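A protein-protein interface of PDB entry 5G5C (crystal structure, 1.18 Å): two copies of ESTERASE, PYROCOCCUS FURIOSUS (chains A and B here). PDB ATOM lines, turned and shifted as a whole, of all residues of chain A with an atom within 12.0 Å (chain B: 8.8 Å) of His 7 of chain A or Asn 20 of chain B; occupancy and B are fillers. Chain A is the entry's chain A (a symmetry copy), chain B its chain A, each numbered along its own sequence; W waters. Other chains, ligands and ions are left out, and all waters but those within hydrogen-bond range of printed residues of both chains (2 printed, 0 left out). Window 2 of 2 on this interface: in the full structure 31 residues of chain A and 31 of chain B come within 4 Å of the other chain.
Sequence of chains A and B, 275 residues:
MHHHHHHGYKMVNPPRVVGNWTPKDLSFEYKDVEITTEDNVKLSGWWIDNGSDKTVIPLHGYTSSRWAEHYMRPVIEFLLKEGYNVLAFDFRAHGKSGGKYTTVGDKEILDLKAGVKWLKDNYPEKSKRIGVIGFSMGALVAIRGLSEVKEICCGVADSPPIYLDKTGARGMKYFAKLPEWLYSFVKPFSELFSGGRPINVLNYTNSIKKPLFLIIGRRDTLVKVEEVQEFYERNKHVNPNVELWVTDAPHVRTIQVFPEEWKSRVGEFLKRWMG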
ATOM      1  N   HIS A   6     -12.589   5.472  19.702  1.00  0.00           N
ATOM      2  CA  HIS A   6     -11.559   6.474  19.453  1.00  0.00           C
ATOM      3  C   HIS A   6     -10.180   5.892  19.759  1.00  0.00           C
ATOM      4  O   HIS A   6     -10.047   5.003  20.600  1.00  0.00           O
ATOM      5  CB  HIS A   6     -11.817   7.730  20.290  1.00  0.00           C
ATOM      6  CG  HIS A   6     -11.163   8.962  19.748  1.00  0.00           C
ATOM      7  ND1 HIS A   6      -9.905   9.371  20.135  1.00  0.00           N
ATOM      8  CD2 HIS A   6     -11.595   9.877  18.847  1.00  0.00           C
ATOM      9  CE1 HIS A   6      -9.590  10.484  19.496  1.00  0.00           C
ATOM     10  NE2 HIS A   6     -10.597  10.814  18.709  1.00  0.00           N
ATOM     11  N   HIS A   7      -9.157   6.394  19.077  1.00  0.00           N
ATOM     12  CA  HIS A   7      -7.821   5.816  19.179  1.00  0.00           C
ATOM     13  C   HIS A   7      -6.887   6.627  20.070  1.00  0.00           C
ATOM     14  O   HIS A   7      -5.748   6.226  20.308  1.00  0.00           O
ATOM     15  CB  HIS A   7      -7.217   5.660  17.783  1.00  0.00           C
ATOM     16  CG  HIS A   7      -7.980   4.716  16.908  1.00  0.00           C
ATOM     17  ND1 HIS A   7      -7.546   3.435  16.636  1.00  0.00           N
ATOM     18  CD2 HIS A   7      -9.164   4.856  16.270  1.00  0.00           C
ATOM     19  CE1 HIS A   7      -8.423   2.834  15.855  1.00  0.00           C
ATOM     20  NE2 HIS A   7      -9.418   3.671  15.621  1.00  0.00           N
ATOM     21  N   GLY A   8      -7.372   7.759  20.566  1.00  0.00           N
ATOM     22  CA  GLY A   8      -6.582   8.598  21.447  1.00  0.00           C
ATOM     23  C   GLY A   8      -5.780   9.642  20.696  1.00  0.00           C
ATOM     24  O   GLY A   8      -5.898   9.774  19.479  1.00  0.00           O
ATOM     25  N   TYR A   9      -4.956  10.383  21.428  1.00  0.00           N
ATOM     26  CA  TYR A   9      -4.168  11.459  20.839  1.00  0.00           C
ATOM     27  C   TYR A   9      -2.682  11.269  21.100  1.00  0.00           C
ATOM     28  O   TYR A   9      -2.252  11.168  22.249  1.00  0.00           O
ATOM     29  CB  TYR A   9      -4.627  12.815  21.381  1.00  0.00           C
ATOM     30  CG  TYR A   9      -6.091  13.096  21.138  1.00  0.00           C
ATOM     31  CD1 TYR A   9      -6.540  13.514  19.893  1.00  0.00           C
ATOM     32  CD2 TYR A   9      -7.026  12.939  22.153  1.00  0.00           C
ATOM     33  CE1 TYR A   9      -7.880  13.767  19.665  1.00  0.00           C
ATOM     34  CE2 TYR A   9      -8.366  13.192  21.934  1.00  0.00           C
ATOM     35  CZ  TYR A   9      -8.787  13.606  20.689  1.00  0.00           C
ATOM     36  OH  TYR A   9     -10.121  13.858  20.465  1.00  0.00           O
ATOM     37  N   LYS A  10      -1.899  11.226  20.028  1.00  0.00           N
ATOM     38  CA  LYS A  10      -0.452  11.117  20.141  1.00  0.00           C
ATOM     39  C   LYS A  10       0.097  12.367  20.814  1.00  0.00           C
ATOM     40  O   LYS A  10       1.108  12.320  21.519  1.00  0.00           O
ATOM     41  CB  LYS A  10       0.187  10.922  18.762  1.00  0.00           C
ATOM     42  CG  LYS A  10       1.708  11.019  18.748  1.00  0.00           C
ATOM     43  CD  LYS A  10       2.224  11.506  17.399  1.00  0.00           C
ATOM     44  CE  LYS A  10       2.961  12.834  17.538  1.00  0.00           C
ATOM     45  NZ  LYS A  10       4.022  12.999  16.503  1.00  0.00           N
ATOM     46  N   MET A  11      -0.505  13.524  20.515  1.00  0.00           N
ATOM     47  CA  MET A  11      -0.029  14.843  20.941  1.00  0.00           C
ATOM     48  C   MET A  11      -1.106  15.934  20.885  1.00  0.00           C
ATOM     49  O   MET A  11      -1.813  16.049  19.916  1.00  0.00           O
ATOM     50  CB  MET A  11       1.159  15.269  20.090  1.00  0.00           C
ATOM     51  CG  MET A  11       1.494  16.709  20.204  1.00  0.00           C
ATOM     52  SD  MET A  11       3.096  16.979  19.453  1.00  0.00           S
ATOM     53  CE  MET A  11       4.278  15.890  20.258  1.00  0.00           C
ATOM     54  N   VAL A  12      -1.243  16.698  21.967  1.00  0.00           N
ATOM     55  CA  VAL A  12      -2.193  17.802  22.001  1.00  0.00           C
ATOM     56  C   VAL A  12      -1.509  19.083  22.457  1.00  0.00           C
ATOM     57  O   VAL A  12      -1.249  19.267  23.648  1.00  0.00           O
ATOM     58  CB  VAL A  12      -3.378  17.497  22.940  1.00  0.00           C
ATOM     59  CG1 VAL A  12      -4.321  18.689  23.021  1.00  0.00           C
ATOM     60  CG2 VAL A  12      -4.123  16.262  22.470  1.00  0.00           C
ATOM     61  N   ASN A  13      -1.203  19.967  21.513  1.00  0.00           N
ATOM     62  CA  ASN A  13      -0.610  21.245  21.872  1.00  0.00           C
ATOM     63  C   ASN A  13      -1.661  22.281  22.212  1.00  0.00           C
ATOM     64  O   ASN A  13      -2.638  22.447  21.478  1.00  0.00           O
ATOM     65  CB  ASN A  13       0.292  21.771  20.756  1.00  0.00           C
ATOM     66  CG  ASN A  13       1.711  21.259  20.874  1.00  0.00           C
ATOM     67  OD1 ASN A  13       1.970  20.277  21.566  1.00  0.00           O
ATOM     68  ND2 ASN A  13       2.643  21.936  20.213  1.00  0.00           N
ATOM     69  N   LYS A 187     -12.497  18.504  23.950  1.00  0.00           N
ATOM     70  CA  LYS A 187     -12.149  17.197  24.506  1.00  0.00           C
ATOM     71  C   LYS A 187     -10.668  16.809  24.521  1.00  0.00           C
ATOM     72  O   LYS A 187     -10.210  16.233  25.507  1.00  0.00           O
ATOM     73  CB  LYS A 187     -12.891  16.076  23.802  1.00  0.00           C
ATOM     74  CG  LYS A 187     -12.593  14.756  24.415  1.00  0.00           C
ATOM     75  CD  LYS A 187     -13.384  13.643  23.729  1.00  0.00           C
ATOM     76  CE  LYS A 187     -13.566  12.461  24.689  1.00  0.00           C
ATOM     77  NZ  LYS A 187     -14.337  11.286  24.130  1.00  0.00           N
ATOM     78  N   PRO A 188      -9.922  17.078  23.432  1.00  0.00           N
ATOM     79  CA  PRO A 188      -8.520  16.644  23.451  1.00  0.00           C
ATOM     80  C   PRO A 188      -7.721  17.184  24.637  1.00  0.00           C
ATOM     81  O   PRO A 188      -6.852  16.484  25.155  1.00  0.00           O
ATOM     82  CB  PRO A 188      -7.967  17.200  22.138  1.00  0.00           C
ATOM     83  CG  PRO A 188      -9.146  17.247  21.236  1.00  0.00           C
ATOM     84  CD  PRO A 188     -10.307  17.614  22.113  1.00  0.00           C
ATOM     85  N   GLU A 191      -8.416  15.146  27.814  1.00  0.00           N
ATOM     86  CA  GLU A 191      -7.706  13.877  27.834  1.00  0.00           C
ATOM     87  C   GLU A 191      -6.204  14.061  28.030  1.00  0.00           C
ATOM     88  O   GLU A 191      -5.566  13.247  28.701  1.00  0.00           O
ATOM     89  CB  GLU A 191      -7.982  13.092  26.550  1.00  0.00           C
ATOM     90  CG  GLU A 191      -9.453  12.822  26.302  1.00  0.00           C
ATOM     91  CD  GLU A 191      -9.676  11.566  25.482  1.00  0.00           C
ATOM     92  OE1 GLU A 191      -8.673  10.963  25.043  1.00  0.00           O
ATOM     93  OE2 GLU A 191     -10.848  11.183  25.278  1.00  0.00           O
ATOM     94  N   LEU A 192      -5.642  15.115  27.441  1.00  0.00           N
ATOM     95  CA  LEU A 192      -4.232  15.424  27.652  1.00  0.00           C
ATOM     96  C   LEU A 192      -4.039  15.637  29.147  1.00  0.00           C
ATOM     97  O   LEU A 192      -3.167  15.025  29.768  1.00  0.00           O
ATOM     98  CB  LEU A 192      -3.795  16.648  26.834  1.00  0.00           C
ATOM     99  CG  LEU A 192      -2.344  17.180  26.916  1.00  0.00           C
ATOM    100  CD1 LEU A 192      -1.954  17.895  28.217  1.00  0.00           C
ATOM    101  CD2 LEU A 192      -1.355  16.076  26.556  1.00  0.00           C
ATOM    102  N   VAL B  17      -4.035  19.312  17.232  1.00  0.00           N
ATOM    103  CA  VAL B  17      -4.502  17.996  17.618  1.00  0.00           C
ATOM    104  C   VAL B  17      -3.934  16.951  16.664  1.00  0.00           C
ATOM    105  O   VAL B  17      -4.152  17.015  15.454  1.00  0.00           O
ATOM    106  CB  VAL B  17      -6.036  17.936  17.623  1.00  0.00           C
ATOM    107  CG1 VAL B  17      -6.514  16.532  17.941  1.00  0.00           C
ATOM    108  CG2 VAL B  17      -6.595  18.942  18.622  1.00  0.00           C
ATOM    109  N   VAL B  18      -3.170  16.014  17.214  1.00  0.00           N
ATOM    110  CA  VAL B  18      -2.597  14.922  16.437  1.00  0.00           C
ATOM    111  C   VAL B  18      -3.162  13.615  16.970  1.00  0.00           C
ATOM    112  O   VAL B  18      -3.003  13.300  18.149  1.00  0.00           O
ATOM    113  CB  VAL B  18      -1.062  14.898  16.510  1.00  0.00           C
ATOM    114  CG1 VAL B  18      -0.514  13.714  15.716  1.00  0.00           C
ATOM    115  CG2 VAL B  18      -0.483  16.216  16.007  1.00  0.00           C
ATOM    116  N   GLY B  19      -3.842  12.867  16.111  1.00  0.00           N
ATOM    117  CA  GLY B  19      -4.494  11.638  16.521  1.00  0.00           C
ATOM    118  C   GLY B  19      -3.556  10.455  16.576  1.00  0.00           C
ATOM    119  O   GLY B  19      -2.370  10.575  16.282  1.00  0.00           O
ATOM    120  N   ASN B  20      -4.100   9.301  16.943  1.00  0.00           N
ATOM    121  CA  ASN B  20      -3.295   8.107  17.145  1.00  0.00           C
ATOM    122  C   ASN B  20      -3.668   7.000  16.161  1.00  0.00           C
ATOM    123  O   ASN B  20      -3.841   5.844  16.545  1.00  0.00           O
ATOM    124  CB  ASN B  20      -3.449   7.617  18.583  1.00  0.00           C
ATOM    125  CG  ASN B  20      -2.269   6.796  19.051  1.00  0.00           C
ATOM    126  OD1 ASN B  20      -1.218   6.773  18.410  1.00  0.00           O
ATOM    127  ND2 ASN B  20      -2.432   6.121  20.183  1.00  0.00           N
ATOM    128  N   TRP B  21      -3.801   7.370  14.892  1.00  0.00           N
ATOM    129  CA  TRP B  21      -4.002   6.406  13.827  1.00  0.00           C
ATOM    130  C   TRP B  21      -3.278   6.918  12.599  1.00  0.00           C
ATOM    131  O   TRP B  21      -3.006   8.120  12.481  1.00  0.00           O
ATOM    132  CB  TRP B  21      -5.487   6.181  13.547  1.00  0.00           C
ATOM    133  CG  TRP B  21      -6.186   7.357  12.930  1.00  0.00           C
ATOM    134  CD1 TRP B  21      -6.805   8.388  13.581  1.00  0.00           C
ATOM    135  CD2 TRP B  21      -6.357   7.609  11.534  1.00  0.00           C
ATOM    136  NE1 TRP B  21      -7.338   9.273  12.673  1.00  0.00           N
ATOM    137  CE2 TRP B  21      -7.078   8.814  11.409  1.00  0.00           C
ATOM    138  CE3 TRP B  21      -5.970   6.930  10.369  1.00  0.00           C
ATOM    139  CZ2 TRP B  21      -7.404   9.359  10.174  1.00  0.00           C
ATOM    140  CZ3 TRP B  21      -6.304   7.478   9.141  1.00  0.00           C
ATOM    141  CH2 TRP B  21      -7.015   8.674   9.055  1.00  0.00           C
ATOM    142  N   THR B  22      -2.943   5.998  11.699  1.00  0.00           N
ATOM    143  CA  THR B  22      -2.314   6.330  10.432  1.00  0.00           C
ATOM    144  C   THR B  22      -2.943   5.457   9.354  1.00  0.00           C
ATOM    145  O   THR B  22      -3.709   4.546   9.667  1.00  0.00           O
ATOM    146  CB  THR B  22      -0.797   6.082  10.436  1.00  0.00           C
ATOM    147  OG1 THR B  22      -0.559   4.672  10.310  1.00  0.00           O
ATOM    148  CG2 THR B  22      -0.123   6.640  11.691  1.00  0.00           C
ATOM    149  N   PRO B  23      -2.621   5.713   8.077  1.00  0.00           N
ATOM    150  CA  PRO B  23      -3.205   4.842   7.054  1.00  0.00           C
ATOM    151  C   PRO B  23      -2.787   3.371   7.194  1.00  0.00           C
ATOM    152  O   PRO B  23      -3.489   2.505   6.657  1.00  0.00           O
ATOM    153  CB  PRO B  23      -2.691   5.456   5.750  1.00  0.00           C
ATOM    154  CG  PRO B  23      -2.521   6.915   6.075  1.00  0.00           C
ATOM    155  CD  PRO B  23      -2.007   6.923   7.489  1.00  0.00           C
ATOM    156  N   ASP B  25      -3.178   1.695   9.785  1.00  0.00           N
ATOM    157  CA  ASP B  25      -4.309   1.138  10.509  1.00  0.00           C
ATOM    158  C   ASP B  25      -5.490   0.800   9.598  1.00  0.00           C
ATOM    159  O   ASP B  25      -6.363   0.025   9.976  1.00  0.00           O
ATOM    160  CB  ASP B  25      -4.737   2.108  11.603  1.00  0.00           C
ATOM    161  CG  ASP B  25      -3.653   2.292  12.646  1.00  0.00           C
ATOM    162  OD1 ASP B  25      -3.142   1.271  13.152  1.00  0.00           O
ATOM    163  OD2 ASP B  25      -3.268   3.438  12.939  1.00  0.00           O
ATOM    164  N   LEU B  26      -5.502   1.383   8.403  1.00  0.00           N
ATOM    165  CA  LEU B  26      -6.472   1.054   7.357  1.00  0.00           C
ATOM    166  C   LEU B  26      -5.922   0.031   6.357  1.00  0.00           C
ATOM    167  O   LEU B  26      -6.598  -0.306   5.378  1.00  0.00           O
ATOM    168  CB  LEU B  26      -6.892   2.314   6.599  1.00  0.00           C
ATOM    169  CG  LEU B  26      -7.329   3.496   7.461  1.00  0.00           C
ATOM    170  CD1 LEU B  26      -7.654   4.705   6.598  1.00  0.00           C
ATOM    171  CD2 LEU B  26      -8.522   3.121   8.321  1.00  0.00           C
ATOM    172  N   TRP B  46       0.127  13.253   4.590  1.00  0.00           N
ATOM    173  CA  TRP B  46       0.286  11.887   4.122  1.00  0.00           C
ATOM    174  C   TRP B  46       0.091  11.830   2.619  1.00  0.00           C
ATOM    175  O   TRP B  46      -0.931  12.295   2.108  1.00  0.00           O
ATOM    176  CB  TRP B  46      -0.742  10.963   4.771  1.00  0.00           C
ATOM    177  CG  TRP B  46      -0.625  10.726   6.237  1.00  0.00           C
ATOM    178  CD1 TRP B  46       0.519  10.659   6.973  1.00  0.00           C
ATOM    179  CD2 TRP B  46      -1.707  10.509   7.148  1.00  0.00           C
ATOM    180  NE1 TRP B  46       0.216  10.395   8.289  1.00  0.00           N
ATOM    181  CE2 TRP B  46      -1.147  10.312   8.423  1.00  0.00           C
ATOM    182  CE3 TRP B  46      -3.098  10.476   7.010  1.00  0.00           C
ATOM    183  CZ2 TRP B  46      -1.927  10.072   9.554  1.00  0.00           C
ATOM    184  CZ3 TRP B  46      -3.873  10.234   8.131  1.00  0.00           C
ATOM    185  CH2 TRP B  46      -3.283  10.032   9.386  1.00  0.00           C
ATOM    186  N   SER B  65      -7.843  18.653  12.198  1.00  0.00           N
ATOM    187  CA  SER B  65      -6.627  18.163  11.549  1.00  0.00           C
ATOM    188  C   SER B  65      -7.011  16.960  10.716  1.00  0.00           C
ATOM    189  O   SER B  65      -8.179  16.550  10.703  1.00  0.00           O
ATOM    190  CB  SER B  65      -5.553  17.771  12.559  1.00  0.00           C
ATOM    191  OG  SER B  65      -5.969  16.627  13.290  1.00  0.00           O
ATOM    192  N   TRP B  67      -6.649  14.003  11.261  1.00  0.00           N
ATOM    193  CA  TRP B  67      -6.980  12.835  12.075  1.00  0.00           C
ATOM    194  C   TRP B  67      -8.439  12.747  12.527  1.00  0.00           C
ATOM    195  O   TRP B  67      -8.844  11.695  13.020  1.00  0.00           O
ATOM    196  CB  TRP B  67      -6.086  12.782  13.330  1.00  0.00           C
ATOM    197  CG  TRP B  67      -4.703  12.290  13.043  1.00  0.00           C
ATOM    198  CD1 TRP B  67      -4.287  10.984  13.013  1.00  0.00           C
ATOM    199  CD2 TRP B  67      -3.554  13.086  12.728  1.00  0.00           C
ATOM    200  NE1 TRP B  67      -2.951  10.922  12.702  1.00  0.00           N
ATOM    201  CE2 TRP B  67      -2.480  12.197  12.515  1.00  0.00           C
ATOM    202  CE3 TRP B  67      -3.326  14.466  12.607  1.00  0.00           C
ATOM    203  CZ2 TRP B  67      -1.204  12.639  12.186  1.00  0.00           C
ATOM    204  CZ3 TRP B  67      -2.069  14.900  12.271  1.00  0.00           C
ATOM    205  CH2 TRP B  67      -1.016  13.991  12.074  1.00  0.00           C
ATOM    206  N   ALA B  68      -9.207  13.836  12.402  1.00  0.00           N
ATOM    207  CA  ALA B  68     -10.528  13.923  13.049  1.00  0.00           C
ATOM    208  C   ALA B  68     -11.342  12.649  12.842  1.00  0.00           C
ATOM    209  O   ALA B  68     -11.693  12.299  11.720  1.00  0.00           O
ATOM    210  CB  ALA B  68     -11.295  15.120  12.523  1.00  0.00           C
ATOM    211  N   GLU B  69     -11.641  11.941  13.923  1.00  0.00           N
ATOM    212  CA  GLU B  69     -12.214  10.614  13.753  1.00  0.00           C
ATOM    213  C   GLU B  69     -13.677  10.632  13.325  1.00  0.00           C
ATOM    214  O   GLU B  69     -14.176   9.633  12.804  1.00  0.00           O
ATOM    215  CB  GLU B  69     -12.047   9.793  15.037  1.00  0.00           C
ATOM    216  CG  GLU B  69     -10.590   9.547  15.403  1.00  0.00           C
ATOM    217  CD  GLU B  69     -10.366   8.205  16.073  1.00  0.00           C
ATOM    218  OE1 GLU B  69     -11.252   7.330  15.971  1.00  0.00           O
ATOM    219  OE2 GLU B  69      -9.302   8.025  16.701  1.00  0.00           O
ATOM    220  N   ARG B  73     -11.162  10.444   9.367  1.00  0.00           N
ATOM    221  CA  ARG B  73     -10.815   9.034   9.259  1.00  0.00           C
ATOM    222  C   ARG B  73     -11.811   8.290   8.346  1.00  0.00           C
ATOM    223  O   ARG B  73     -11.379   7.573   7.442  1.00  0.00           O
ATOM    224  CB  ARG B  73     -10.720   8.380  10.644  1.00  0.00           C
ATOM    225  CG  ARG B  73     -10.100   6.988  10.573  1.00  0.00           C
ATOM    226  CD  ARG B  73     -10.058   6.287  11.927  1.00  0.00           C
ATOM    227  NE  ARG B  73      -9.869   4.844  11.762  1.00  0.00           N
ATOM    228  CZ  ARG B  73      -8.960   4.118  12.404  1.00  0.00           C
ATOM    229  NH1 ARG B  73      -8.156   4.690  13.282  1.00  0.00           N
ATOM    230  NH2 ARG B  73      -8.868   2.815  12.177  1.00  0.00           N
HETATM  231  O   HOH W   1     -10.815  12.756  16.573  1.00  0.00           O
HETATM  232  O   HOH W   2      -7.287   9.620  17.033  1.00  0.00           O
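The backbone carbonyl oxygen (O) of His 7 of chain A sits close to the side-chain amide nitrogen (ND2) of Asn 20 of chain B, 3.3 Å away.
The backbone carbonyl oxygen (O) of Val 18 of chain B is in hydrogen-bond range of the backbone NH (N) of Lys 10 of chain A.
The backbone NH (N) of Asn 20 of chain B lies within hydrogen-bond range of the backbone carbonyl oxygen (O) of Gly 8 of chain A (3.1 Å).
The side-chain carboxylate (OE2) of Glu 69 of chain B is in hydrogen-bond range of the backbone NH (N) of His 7 of chain A.
The backbone NH (N) of Val 18 of chain B sits at hydrogen-bond distance from the backbone carbonyl oxygen (O) of Met 11 of chain A.
A ring nitrogen (NE2) of His 7 of chain A lies within hydrogen-bond range of the guanidinium group (NH1) of Arg 73 of chain B, 2.8 Å away.
The backbone carbonyl oxygen (O) of Ala 68 of chain B sits at hydrogen-bond distance from the backbone NH (N) of Arg 73 of chain B (3.0 Å).
N of Gly 8 of chain A is in hydrogen-bond range of ND1 of His 6 of chain A (3.0 Å).
OG of Ser 65 of chain B sits at hydrogen-bond distance from O of Val 17 of chain B (2.9 Å).
His 6 of chain A touches Glu 69 of chain B (CD2 to CD, 3.5 Å).
Gly 8 of chain A touches Gly 19 of chain B (O to CA, 3.8 Å).
CE1 of Tyr 9 of chain A touches CG1 of Val 17 of chain B (3.5 Å).
CA of Tyr 9 of chain A touches O of Val 18 of chain B, at 3.5 Å.
Lys 10 of chain A touches Gly 19 of chain B.
O of Met 11 of chain A touches C of Val 17 of chain B, at 3.99 Å.
Of the printed residues of chain B, His 7 of chain A touches Asn 20, Glu 69 and Arg 73.
Asn 20 of chain B touches just these residues of chain A: His 7 (3.2 Å) and Gly 8 (3.1 Å).
Gly 8 of chain A touches two residues of chain B.
Of chain A, only Tyr 9, Lys 10 and Met 11 come within 4 Å of Val 18 of chain B.
Gly 19 of chain B touches just these residues of chain A: Gly 8 (3.8 Å) and Lys 10 (3.6 Å).
No residue of chain A comes within 4 Å of Trp 67 of chain B.
Of chain A, only His 6 and His 7 come within 4 Å of Glu 69 of chain B.
Printed residues of chain B within 4 Å of Tyr 9 of chain A: Val 17 and Val 18.
Printed residues of chain A within 4 Å of Val 17 of chain B: Tyr 9 (3.5 Å) and Met 11 (3.99 Å).
Of the printed residues of chain A, Arg 73 of chain B touches His 7 (2.8 Å).
Of the printed residues of chain B, Met 11 of chain A touches Val 17 (3.99 Å) and Val 18 (3.0 Å).
Printed residues of chain B within 4 Å of Lys 10 of chain A: Val 18 (3.0 Å) and Gly 19 (3.6 Å).
The nearest residue of chain B that does not touch His 7 of chain A is Trp 21 of chain B (4.4 Å).
Hydrophobic or aromatic side chains of chain B that line the printed part of chain A: Val 17 and Val 18.
Along chain B the printed residues that touch a printed residue of chain A span positions 17 to 73.
Of the 12 printed residues of chain A, 6 touch a printed residue of chain B.
Printed residues of chain A that touch a printed residue of chain B: His 6, His 7, Gly 8, Tyr 9, Lys 10 and Met 11.
Hydrophobic or aromatic side chains of chain A within 4 Å of the printed part of chain B: His 6, His 7 and Tyr 9.
Among the printed residues, 12 pairs touch across the chains.
Among the printed residues, no Asp or Glu carboxylate lies within 4 Å of a Lys or Arg side-chain nitrogen of the other chain.
No position is printed for both chains.
Of the 12 pairs that touch across the chains among the printed residues, none has its exchanged pair printed and touching as well.
Water W2 lies within hydrogen-bond range of the side-chain carboxylate of Glu 69 of chain B (2.6 Å), the backbone carbonyl oxygen of Gly 8 of chain A (2.8 Å) and the backbone NH of Asn 20 of chain B (3.2 Å).
Water W1 bridges N of Glu 69 of chain B and NE2 of His 6 of chain A.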
